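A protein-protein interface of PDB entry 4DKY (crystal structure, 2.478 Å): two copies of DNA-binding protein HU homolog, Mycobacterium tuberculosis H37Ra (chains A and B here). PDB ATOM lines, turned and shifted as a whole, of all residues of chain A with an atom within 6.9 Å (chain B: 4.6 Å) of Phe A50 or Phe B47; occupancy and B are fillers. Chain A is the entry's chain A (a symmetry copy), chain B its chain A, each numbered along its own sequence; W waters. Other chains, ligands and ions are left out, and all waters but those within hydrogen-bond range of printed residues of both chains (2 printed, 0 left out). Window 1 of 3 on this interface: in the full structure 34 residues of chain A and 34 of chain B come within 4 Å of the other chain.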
ATOM      1  N   VAL A  28      12.291  26.454 -38.972  1.00  0.00           N
ATOM      2  CA  VAL A  28      13.161  25.500 -38.202  1.00  0.00           C
ATOM      3  C   VAL A  28      12.968  25.642 -36.669  1.00  0.00           C
ATOM      4  O   VAL A  28      12.611  24.722 -35.963  1.00  0.00           O
ATOM      5  CB  VAL A  28      14.631  25.745 -38.472  1.00  0.00           C
ATOM      6  CG1 VAL A  28      15.409  25.058 -37.379  1.00  0.00           C
ATOM      7  CG2 VAL A  28      15.024  25.062 -39.790  1.00  0.00           C
ATOM      8  N   VAL A  29      13.196  26.868 -36.202  1.00  0.00           N
ATOM      9  CA  VAL A  29      12.903  27.314 -34.864  1.00  0.00           C
ATOM     10  C   VAL A  29      11.538  26.941 -34.337  1.00  0.00           C
ATOM     11  O   VAL A  29      11.420  26.156 -33.382  1.00  0.00           O
ATOM     12  CB  VAL A  29      12.970  28.845 -34.819  1.00  0.00           C
ATOM     13  CG1 VAL A  29      12.205  29.285 -33.639  1.00  0.00           C
ATOM     14  CG2 VAL A  29      14.480  29.316 -34.790  1.00  0.00           C
ATOM     15  N   ASP A  30      10.521  27.390 -35.028  1.00  0.00           N
ATOM     16  CA  ASP A  30       9.157  27.060 -34.722  1.00  0.00           C
ATOM     17  C   ASP A  30       8.914  25.612 -34.642  1.00  0.00           C
ATOM     18  O   ASP A  30       8.216  25.155 -33.702  1.00  0.00           O
ATOM     19  CB  ASP A  30       8.246  27.693 -35.784  1.00  0.00           C
ATOM     20  CG  ASP A  30       6.780  27.478 -35.479  1.00  0.00           C
ATOM     21  OD1 ASP A  30       6.374  26.560 -34.722  1.00  0.00           O
ATOM     22  OD2 ASP A  30       5.991  28.278 -35.996  1.00  0.00           O
ATOM     23  N   ILE A  32      11.066  23.140 -33.986  1.00  0.00           N
ATOM     24  CA  ILE A  32      11.704  22.517 -32.901  1.00  0.00           C
ATOM     25  C   ILE A  32      10.914  22.846 -31.649  1.00  0.00           C
ATOM     26  O   ILE A  32      10.500  21.953 -30.940  1.00  0.00           O
ATOM     27  CB  ILE A  32      13.142  23.075 -32.816  1.00  0.00           C
ATOM     28  CG1 ILE A  32      13.914  22.634 -34.111  1.00  0.00           C
ATOM     29  CG2 ILE A  32      13.756  22.736 -31.503  1.00  0.00           C
ATOM     30  CD1 ILE A  32      15.318  23.202 -34.088  1.00  0.00           C
ATOM     31  N   VAL A  33      10.659  24.170 -31.416  1.00  0.00           N
ATOM     32  CA  VAL A  33       9.892  24.587 -30.260  1.00  0.00           C
ATOM     33  C   VAL A  33       8.619  23.723 -30.153  1.00  0.00           C
ATOM     34  O   VAL A  33       8.198  23.259 -29.064  1.00  0.00           O
ATOM     35  CB  VAL A  33       9.540  26.032 -30.347  1.00  0.00           C
ATOM     36  CG1 VAL A  33       8.714  26.464 -29.120  1.00  0.00           C
ATOM     37  CG2 VAL A  33      10.821  26.870 -30.464  1.00  0.00           C
ATOM     38  N   ALA A  35       8.051  20.744 -31.204  1.00  0.00           N
ATOM     39  CA  ALA A  35       8.218  19.266 -30.884  1.00  0.00           C
ATOM     40  C   ALA A  35       8.563  19.128 -29.407  1.00  0.00           C
ATOM     41  O   ALA A  35       8.137  18.249 -28.701  1.00  0.00           O
ATOM     42  CB  ALA A  35       9.232  18.589 -31.777  1.00  0.00           C
ATOM     43  N   VAL A  36       9.374  20.003 -28.938  1.00  0.00           N
ATOM     44  CA  VAL A  36       9.782  19.851 -27.585  1.00  0.00           C
ATOM     45  C   VAL A  36       8.560  20.197 -26.681  1.00  0.00           C
ATOM     46  O   VAL A  36       8.400  19.617 -25.614  1.00  0.00           O
ATOM     47  CB  VAL A  36      10.983  20.814 -27.285  1.00  0.00           C
ATOM     48  CG1 VAL A  36      11.152  21.008 -25.776  1.00  0.00           C
ATOM     49  CG2 VAL A  36      12.255  20.398 -28.093  1.00  0.00           C
ATOM     50  N   ASP A  40       8.266  15.929 -27.379  1.00  0.00           N
ATOM     51  CA  ASP A  40       9.109  15.163 -28.248  1.00  0.00           C
ATOM     52  C   ASP A  40      10.532  15.666 -28.228  1.00  0.00           C
ATOM     53  O   ASP A  40      10.809  16.740 -27.656  1.00  0.00           O
ATOM     54  CB  ASP A  40       8.627  15.290 -29.613  1.00  0.00           C
ATOM     55  CG  ASP A  40       8.127  14.010 -30.096  1.00  0.00           C
ATOM     56  OD1 ASP A  40       7.788  13.170 -29.196  1.00  0.00           O
ATOM     57  OD2 ASP A  40       8.175  13.795 -31.361  1.00  0.00           O
ATOM     58  N   SER A  41      11.435  14.924 -28.873  1.00  0.00           N
ATOM     59  CA  SER A  41      12.854  15.281 -28.876  1.00  0.00           C
ATOM     60  C   SER A  41      13.242  15.646 -30.268  1.00  0.00           C
ATOM     61  O   SER A  41      12.795  15.010 -31.208  1.00  0.00           O
ATOM     62  CB  SER A  41      13.650  14.049 -28.427  1.00  0.00           C
ATOM     63  OG  SER A  41      14.889  14.409 -27.870  1.00  0.00           O
ATOM     64  N   VAL A  42      14.113  16.624 -30.450  1.00  0.00           N
ATOM     65  CA  VAL A  42      14.686  16.854 -31.808  1.00  0.00           C
ATOM     66  C   VAL A  42      16.180  16.606 -31.830  1.00  0.00           C
ATOM     67  O   VAL A  42      16.986  17.335 -31.236  1.00  0.00           O
ATOM     68  CB  VAL A  42      14.404  18.224 -32.363  1.00  0.00           C
ATOM     69  CG1 VAL A  42      15.036  18.298 -33.768  1.00  0.00           C
ATOM     70  CG2 VAL A  42      12.867  18.444 -32.342  1.00  0.00           C
ATOM     71  N   THR A  43      16.521  15.552 -32.530  1.00  0.00           N
ATOM     72  CA  THR A  43      17.898  15.133 -32.679  1.00  0.00           C
ATOM     73  C   THR A  43      18.488  15.505 -34.050  1.00  0.00           C
ATOM     74  O   THR A  43      18.110  14.948 -35.078  1.00  0.00           O
ATOM     75  CB  THR A  43      17.978  13.604 -32.659  1.00  0.00           C
ATOM     76  OG1 THR A  43      17.098  13.070 -31.618  1.00  0.00           O
ATOM     77  CG2 THR A  43      19.477  13.222 -32.511  1.00  0.00           C
ATOM     78  N   ILE A  44      19.480  16.346 -34.079  1.00  0.00           N
ATOM     79  CA  ILE A  44      20.061  16.662 -35.353  1.00  0.00           C
ATOM     80  C   ILE A  44      21.487  16.244 -35.376  1.00  0.00           C
ATOM     81  O   ILE A  44      22.266  16.737 -34.642  1.00  0.00           O
ATOM     82  CB  ILE A  44      19.980  18.159 -35.660  1.00  0.00           C
ATOM     83  CG1 ILE A  44      18.623  18.691 -35.269  1.00  0.00           C
ATOM     84  CG2 ILE A  44      20.221  18.393 -37.108  1.00  0.00           C
ATOM     85  CD1 ILE A  44      18.460  20.149 -35.538  1.00  0.00           C
ATOM     86  N   PHE A  47      24.821  18.133 -34.689  1.00  0.00           N
ATOM     87  CA  PHE A  47      24.480  19.356 -34.008  1.00  0.00           C
ATOM     88  C   PHE A  47      24.230  19.018 -32.585  1.00  0.00           C
ATOM     89  O   PHE A  47      25.036  19.216 -31.774  1.00  0.00           O
ATOM     90  CB  PHE A  47      23.240  19.967 -34.629  1.00  0.00           C
ATOM     91  CG  PHE A  47      23.030  21.393 -34.280  1.00  0.00           C
ATOM     92  CD1 PHE A  47      24.054  22.277 -34.325  1.00  0.00           C
ATOM     93  CD2 PHE A  47      21.776  21.846 -33.972  1.00  0.00           C
ATOM     94  CE1 PHE A  47      23.847  23.583 -34.026  1.00  0.00           C
ATOM     95  CE2 PHE A  47      21.563  23.140 -33.673  1.00  0.00           C
ATOM     96  CZ  PHE A  47      22.605  24.010 -33.685  1.00  0.00           C
ATOM     97  N   GLY A  48      23.084  18.473 -32.312  1.00  0.00           N
ATOM     98  CA  GLY A  48      22.767  18.145 -30.981  1.00  0.00           C
ATOM     99  C   GLY A  48      21.332  17.812 -30.913  1.00  0.00           C
ATOM    100  O   GLY A  48      20.681  17.733 -31.876  1.00  0.00           O
ATOM    101  N   VAL A  49      20.859  17.634 -29.710  1.00  0.00           N
ATOM    102  CA  VAL A  49      19.444  17.348 -29.506  1.00  0.00           C
ATOM    103  C   VAL A  49      18.766  18.340 -28.597  1.00  0.00           C
ATOM    104  O   VAL A  49      19.327  18.857 -27.595  1.00  0.00           O
ATOM    105  CB  VAL A  49      19.184  15.920 -29.033  1.00  0.00           C
ATOM    106  CG1 VAL A  49      20.419  15.068 -28.939  1.00  0.00           C
ATOM    107  CG2 VAL A  49      18.463  15.987 -27.824  1.00  0.00           C
ATOM    108  N   PHE A  50      17.544  18.639 -28.981  1.00  0.00           N
ATOM    109  CA  PHE A  50      16.644  19.454 -28.161  1.00  0.00           C
ATOM    110  C   PHE A  50      15.638  18.536 -27.492  1.00  0.00           C
ATOM    111  O   PHE A  50      15.088  17.647 -28.097  1.00  0.00           O
ATOM    112  CB  PHE A  50      15.939  20.532 -28.989  1.00  0.00           C
ATOM    113  CG  PHE A  50      16.891  21.450 -29.688  1.00  0.00           C
ATOM    114  CD1 PHE A  50      17.271  22.638 -29.113  1.00  0.00           C
ATOM    115  CD2 PHE A  50      17.413  21.113 -30.990  1.00  0.00           C
ATOM    116  CE1 PHE A  50      18.153  23.498 -29.783  1.00  0.00           C
ATOM    117  CE2 PHE A  50      18.292  21.974 -31.699  1.00  0.00           C
ATOM    118  CZ  PHE A  50      18.654  23.142 -31.105  1.00  0.00           C
ATOM    119  N   GLU A  51      15.435  18.768 -26.216  1.00  0.00           N
ATOM    120  CA  GLU A  51      14.564  17.924 -25.468  1.00  0.00           C
ATOM    121  C   GLU A  51      13.842  18.761 -24.411  1.00  0.00           C
ATOM    122  O   GLU A  51      14.249  19.867 -24.016  1.00  0.00           O
ATOM    123  CB  GLU A  51      15.344  16.754 -24.889  1.00  0.00           C
ATOM    124  CG  GLU A  51      16.524  17.194 -24.047  1.00  0.00           C
ATOM    125  CD  GLU A  51      17.425  16.074 -23.616  1.00  0.00           C
ATOM    126  OE1 GLU A  51      17.138  14.933 -23.997  1.00  0.00           O
ATOM    127  OE2 GLU A  51      18.433  16.350 -22.905  1.00  0.00           O
ATOM    128  N   GLN A  52      12.721  18.195 -24.012  1.00  0.00           N
ATOM    129  CA  GLN A  52      12.006  18.680 -22.840  1.00  0.00           C
ATOM    130  C   GLN A  52      12.605  17.909 -21.588  1.00  0.00           C
ATOM    131  O   GLN A  52      12.893  16.707 -21.679  1.00  0.00           O
ATOM    132  CB  GLN A  52      10.510  18.403 -23.043  1.00  0.00           C
ATOM    133  CG  GLN A  52       9.709  18.240 -21.814  1.00  0.00           C
ATOM    134  CD  GLN A  52       8.215  18.413 -22.045  1.00  0.00           C
ATOM    135  OE1 GLN A  52       7.746  19.168 -22.924  1.00  0.00           O
ATOM    136  NE2 GLN A  52       7.432  17.699 -21.245  1.00  0.00           N
ATOM    137  N   PRO A  77      12.957  23.408 -21.513  1.00  0.00           N
ATOM    138  CA  PRO A  77      13.616  22.969 -22.742  1.00  0.00           C
ATOM    139  C   PRO A  77      15.127  22.786 -22.541  1.00  0.00           C
ATOM    140  O   PRO A  77      15.735  23.459 -21.729  1.00  0.00           O
ATOM    141  CB  PRO A  77      13.292  24.158 -23.713  1.00  0.00           C
ATOM    142  CG  PRO A  77      13.058  25.297 -22.830  1.00  0.00           C
ATOM    143  CD  PRO A  77      12.718  24.827 -21.486  1.00  0.00           C
ATOM    144  N   ALA A  78      15.772  21.968 -23.315  1.00  0.00           N
ATOM    145  CA  ALA A  78      17.256  21.978 -23.155  1.00  0.00           C
ATOM    146  C   ALA A  78      17.989  21.454 -24.398  1.00  0.00           C
ATOM    147  O   ALA A  78      17.350  20.739 -25.217  1.00  0.00           O
ATOM    148  CB  ALA A  78      17.660  21.158 -21.871  1.00  0.00           C
ATOM    149  N   PHE A  79      19.293  21.788 -24.564  1.00  0.00           N
ATOM    150  CA  PHE A  79      20.074  21.293 -25.791  1.00  0.00           C
ATOM    151  C   PHE A  79      21.384  20.581 -25.343  1.00  0.00           C
ATOM    152  O   PHE A  79      22.257  21.220 -24.685  1.00  0.00           O
ATOM    153  CB  PHE A  79      20.439  22.463 -26.645  1.00  0.00           C
ATOM    154  CG  PHE A  79      21.298  22.167 -27.808  1.00  0.00           C
ATOM    155  CD1 PHE A  79      20.811  21.542 -28.964  1.00  0.00           C
ATOM    156  CD2 PHE A  79      22.588  22.634 -27.857  1.00  0.00           C
ATOM    157  CE1 PHE A  79      21.646  21.309 -30.086  1.00  0.00           C
ATOM    158  CE2 PHE A  79      23.396  22.396 -28.997  1.00  0.00           C
ATOM    159  CZ  PHE A  79      22.937  21.694 -30.080  1.00  0.00           C
ATOM    160  N   ARG A  80      21.528  19.319 -25.701  1.00  0.00           N
ATOM    161  CA  ARG A  80      22.771  18.659 -25.595  1.00  0.00           C
ATOM    162  C   ARG A  80      23.585  18.658 -26.866  1.00  0.00           C
ATOM    163  O   ARG A  80      23.270  17.871 -27.810  1.00  0.00           O
ATOM    164  CB  ARG A  80      22.460  17.188 -25.356  1.00  0.00           C
ATOM    165  CG  ARG A  80      22.190  16.953 -23.939  1.00  0.00           C
ATOM    166  CD  ARG A  80      22.296  15.510 -23.732  1.00  0.00           C
ATOM    167  NE  ARG A  80      21.067  14.781 -24.044  1.00  0.00           N
ATOM    168  CZ  ARG A  80      20.997  13.885 -25.012  1.00  0.00           C
ATOM    169  NH1 ARG A  80      21.991  13.632 -25.795  1.00  0.00           N
ATOM    170  NH2 ARG A  80      19.952  13.188 -25.194  1.00  0.00           N
ATOM    171  N   ILE B  44      19.217  33.939 -31.138  1.00  0.00           N
ATOM    172  CA  ILE B  44      18.044  33.966 -31.965  1.00  0.00           C
ATOM    173  C   ILE B  44      16.846  34.253 -31.134  1.00  0.00           C
ATOM    174  O   ILE B  44      16.511  33.502 -30.289  1.00  0.00           O
ATOM    175  CB  ILE B  44      17.833  32.638 -32.695  1.00  0.00           C
ATOM    176  CG1 ILE B  44      19.151  32.129 -33.227  1.00  0.00           C
ATOM    177  CG2 ILE B  44      16.870  32.822 -33.813  1.00  0.00           C
ATOM    178  CD1 ILE B  44      19.032  30.834 -33.958  1.00  0.00           C
ATOM    179  N   THR B  45      16.199  35.362 -31.403  1.00  0.00           N
ATOM    180  CA  THR B  45      15.115  35.788 -30.541  1.00  0.00           C
ATOM    181  C   THR B  45      13.923  34.870 -30.616  1.00  0.00           C
ATOM    182  O   THR B  45      13.471  34.501 -31.684  1.00  0.00           O
ATOM    183  CB  THR B  45      14.680  37.222 -30.841  1.00  0.00           C
ATOM    184  OG1 THR B  45      14.384  37.346 -32.244  1.00  0.00           O
ATOM    185  CG2 THR B  45      15.799  38.159 -30.445  1.00  0.00           C
ATOM    186  N   GLY B  46      13.428  34.509 -29.451  1.00  0.00           N
ATOM    187  CA  GLY B  46      12.372  33.536 -29.388  1.00  0.00           C
ATOM    188  C   GLY B  46      12.886  32.133 -29.433  1.00  0.00           C
ATOM    189  O   GLY B  46      12.119  31.195 -29.481  1.00  0.00           O
ATOM    190  N   PHE B  47      14.183  31.975 -29.437  1.00  0.00           N
ATOM    191  CA  PHE B  47      14.721  30.639 -29.421  1.00  0.00           C
ATOM    192  C   PHE B  47      15.687  30.561 -28.298  1.00  0.00           C
ATOM    193  O   PHE B  47      15.394  30.067 -27.290  1.00  0.00           O
ATOM    194  CB  PHE B  47      15.416  30.342 -30.735  1.00  0.00           C
ATOM    195  CG  PHE B  47      15.655  28.899 -30.979  1.00  0.00           C
ATOM    196  CD1 PHE B  47      14.682  27.987 -30.755  1.00  0.00           C
ATOM    197  CD2 PHE B  47      16.849  28.482 -31.503  1.00  0.00           C
ATOM    198  CE1 PHE B  47      14.903  26.672 -31.003  1.00  0.00           C
ATOM    199  CE2 PHE B  47      17.076  27.180 -31.751  1.00  0.00           C
ATOM    200  CZ  PHE B  47      16.105  26.268 -31.487  1.00  0.00           C
ATOM    201  N   GLY B  48      16.854  31.095 -28.500  1.00  0.00           N
ATOM    202  CA  GLY B  48      17.830  31.041 -27.489  1.00  0.00           C
ATOM    203  C   GLY B  48      19.122  31.457 -28.066  1.00  0.00           C
ATOM    204  O   GLY B  48      19.195  31.871 -29.153  1.00  0.00           O
ATOM    205  N   PHE B  50      23.281  30.415 -28.678  1.00  0.00           N
ATOM    206  CA  PHE B  50      24.402  29.471 -28.713  1.00  0.00           C
ATOM    207  C   PHE B  50      25.681  30.232 -28.414  1.00  0.00           C
ATOM    208  O   PHE B  50      25.918  31.303 -28.921  1.00  0.00           O
ATOM    209  CB  PHE B  50      24.496  28.748 -30.059  1.00  0.00           C
ATOM    210  CG  PHE B  50      23.247  28.002 -30.410  1.00  0.00           C
ATOM    211  CD1 PHE B  50      23.116  26.670 -30.102  1.00  0.00           C
ATOM    212  CD2 PHE B  50      22.165  28.663 -31.098  1.00  0.00           C
ATOM    213  CE1 PHE B  50      21.948  25.975 -30.448  1.00  0.00           C
ATOM    214  CE2 PHE B  50      20.980  27.979 -31.477  1.00  0.00           C
ATOM    215  CZ  PHE B  50      20.875  26.662 -31.157  1.00  0.00           C
ATOM    216  N   PHE B  79      23.772  25.970 -25.143  1.00  0.00           N
ATOM    217  CA  PHE B  79      22.519  26.738 -25.592  1.00  0.00           C
ATOM    218  C   PHE B  79      21.684  27.175 -24.353  1.00  0.00           C
ATOM    219  O   PHE B  79      21.218  26.300 -23.564  1.00  0.00           O
ATOM    220  CB  PHE B  79      21.674  25.846 -26.442  1.00  0.00           C
ATOM    221  CG  PHE B  79      20.370  26.399 -26.857  1.00  0.00           C
ATOM    222  CD1 PHE B  79      20.251  27.375 -27.856  1.00  0.00           C
ATOM    223  CD2 PHE B  79      19.202  25.862 -26.377  1.00  0.00           C
ATOM    224  CE1 PHE B  79      18.983  27.858 -28.269  1.00  0.00           C
ATOM    225  CE2 PHE B  79      17.949  26.358 -26.817  1.00  0.00           C
ATOM    226  CZ  PHE B  79      17.849  27.382 -27.720  1.00  0.00           C
ATOM    227  N   ARG B  80      21.483  28.469 -24.197  1.00  0.00           N
ATOM    228  CA  ARG B  80      20.527  28.964 -23.283  1.00  0.00           C
ATOM    229  C   ARG B  80      19.182  29.272 -23.897  1.00  0.00           C
ATOM    230  O   ARG B  80      19.037  30.326 -24.588  1.00  0.00           O
ATOM    231  CB  ARG B  80      21.037  30.320 -22.815  1.00  0.00           C
ATOM    232  CG  ARG B  80      22.009  30.148 -21.738  1.00  0.00           C
ATOM    233  CD  ARG B  80      22.144  31.452 -21.091  1.00  0.00           C
ATOM    234  NE  ARG B  80      23.099  32.340 -21.754  1.00  0.00           N
ATOM    235  CZ  ARG B  80      22.739  33.484 -22.308  1.00  0.00           C
ATOM    236  NH1 ARG B  80      21.510  33.873 -22.360  1.00  0.00           N
ATOM    237  NH2 ARG B  80      23.600  34.288 -22.782  1.00  0.00           N
ATOM    238  N   PRO B  81      18.166  28.467 -23.627  1.00  0.00           N
ATOM    239  CA  PRO B  81      16.811  28.673 -24.158  1.00  0.00           C
ATOM    240  C   PRO B  81      16.219  29.946 -23.763  1.00  0.00           C
ATOM    241  O   PRO B  81      16.188  30.309 -22.565  1.00  0.00           O
ATOM    242  CB  PRO B  81      16.015  27.570 -23.507  1.00  0.00           C
ATOM    243  CG  PRO B  81      16.868  27.156 -22.350  1.00  0.00           C
ATOM    244  CD  PRO B  81      18.243  27.235 -22.873  1.00  0.00           C
ATOM    245  N   GLY B  82      15.730  30.681 -24.728  1.00  0.00           N
ATOM    246  CA  GLY B  82      15.210  32.013 -24.403  1.00  0.00           C
ATOM    247  C   GLY B  82      13.859  31.988 -23.689  1.00  0.00           C
ATOM    248  O   GLY B  82      13.158  30.945 -23.691  1.00  0.00           O
ATOM    249  N   PHE B  85      10.769  30.529 -25.413  1.00  0.00           N
ATOM    250  CA  PHE B  85      10.860  29.063 -25.538  1.00  0.00           C
ATOM    251  C   PHE B  85      10.532  28.432 -24.151  1.00  0.00           C
ATOM    252  O   PHE B  85       9.696  27.525 -24.037  1.00  0.00           O
ATOM    253  CB  PHE B  85      12.288  28.735 -25.954  1.00  0.00           C
ATOM    254  CG  PHE B  85      12.478  27.352 -26.417  1.00  0.00           C
ATOM    255  CD1 PHE B  85      11.450  26.431 -26.304  1.00  0.00           C
ATOM    256  CD2 PHE B  85      13.750  26.933 -26.949  1.00  0.00           C
ATOM    257  CE1 PHE B  85      11.636  25.117 -26.749  1.00  0.00           C
ATOM    258  CE2 PHE B  85      13.955  25.636 -27.394  1.00  0.00           C
ATOM    259  CZ  PHE B  85      12.910  24.703 -27.320  1.00  0.00           C
HETATM  260  O   HOH W   1      19.950  23.802 -22.979  1.00  0.00           O
HETATM  261  O   HOH W   2      23.849  23.531 -24.121  1.00  0.00           O
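Of chain B, only Phe B47 comes within 4 Å of Phe A50. Of the printed residues of chain A, Phe B47 touches Phe A50 (3.8 Å). Printed residues of chain A within 4 Å of Phe B85: Val A33 and Pro A77. Of the printed residues of chain B, Pro A77 touches Pro B81 and Phe B85. Ala A78 touches none of the printed residues of chain B.
The backbone carbonyl oxygen (O) of Phe B47 is in hydrogen-bond range of the backbone NH (N) of Gly B82 (2.7 Å). OG of Ser A41 sits at hydrogen-bond distance from O of Phe A50, at 3.3 Å. The backbone carbonyl oxygen (O) of Val A42 sits at hydrogen-bond distance from the backbone NH (N) of Phe A50, 2.7 Å away.
Of the 22 printed residues of chain A, 5 touch a printed residue of chain B. Printed residues of chain A that touch a printed residue of chain B: Val A33, Phe A47, Phe A50, Pro A77 and Phe A79. Hydrophobic or aromatic side chains of chain A within 4 Å of the printed part of chain B: Val A33, Phe A47, Phe A50, Pro A77 and Phe A79. Hydrophobic or aromatic side chains of chain B within 4 Å of the printed part of chain A: Phe B47, Phe B50, Phe B79, Pro B81 and Phe B85. Among the printed residues, 6 pairs touch across the chains.
Phe A47 touches Phe B50, and with the chains exchanged Phe A50 touches Phe B47. Phe A79 touches its own counterpart, Phe B79. Positions printed for both chains: 44, 47, 48, 50, 79 and 80. Of the 6 pairs that touch across the chains among the printed residues, 3 have their exchanged pair printed and touching as well.
Val A33 touches Phe B85. Phe B50 touches Phe A47 (CE1 to CZ, 3.8 Å). CE1 of Phe A50 touches CZ of Phe B47, 3.8 Å away. Pro B81 touches Pro A77 (CB to CG, 3.8 Å). Phe B85 touches Pro A77. CB of Phe A79 touches CB of Phe B79, 3.6 Å away.
Water W2 lies within hydrogen-bond range of N of Phe B79 (2.6 Å) and O of Phe A79 (2.9 Å). Water W1 lies within hydrogen-bond range of N of Phe A79 (2.6 Å) and O of Phe B79 (2.9 Å).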
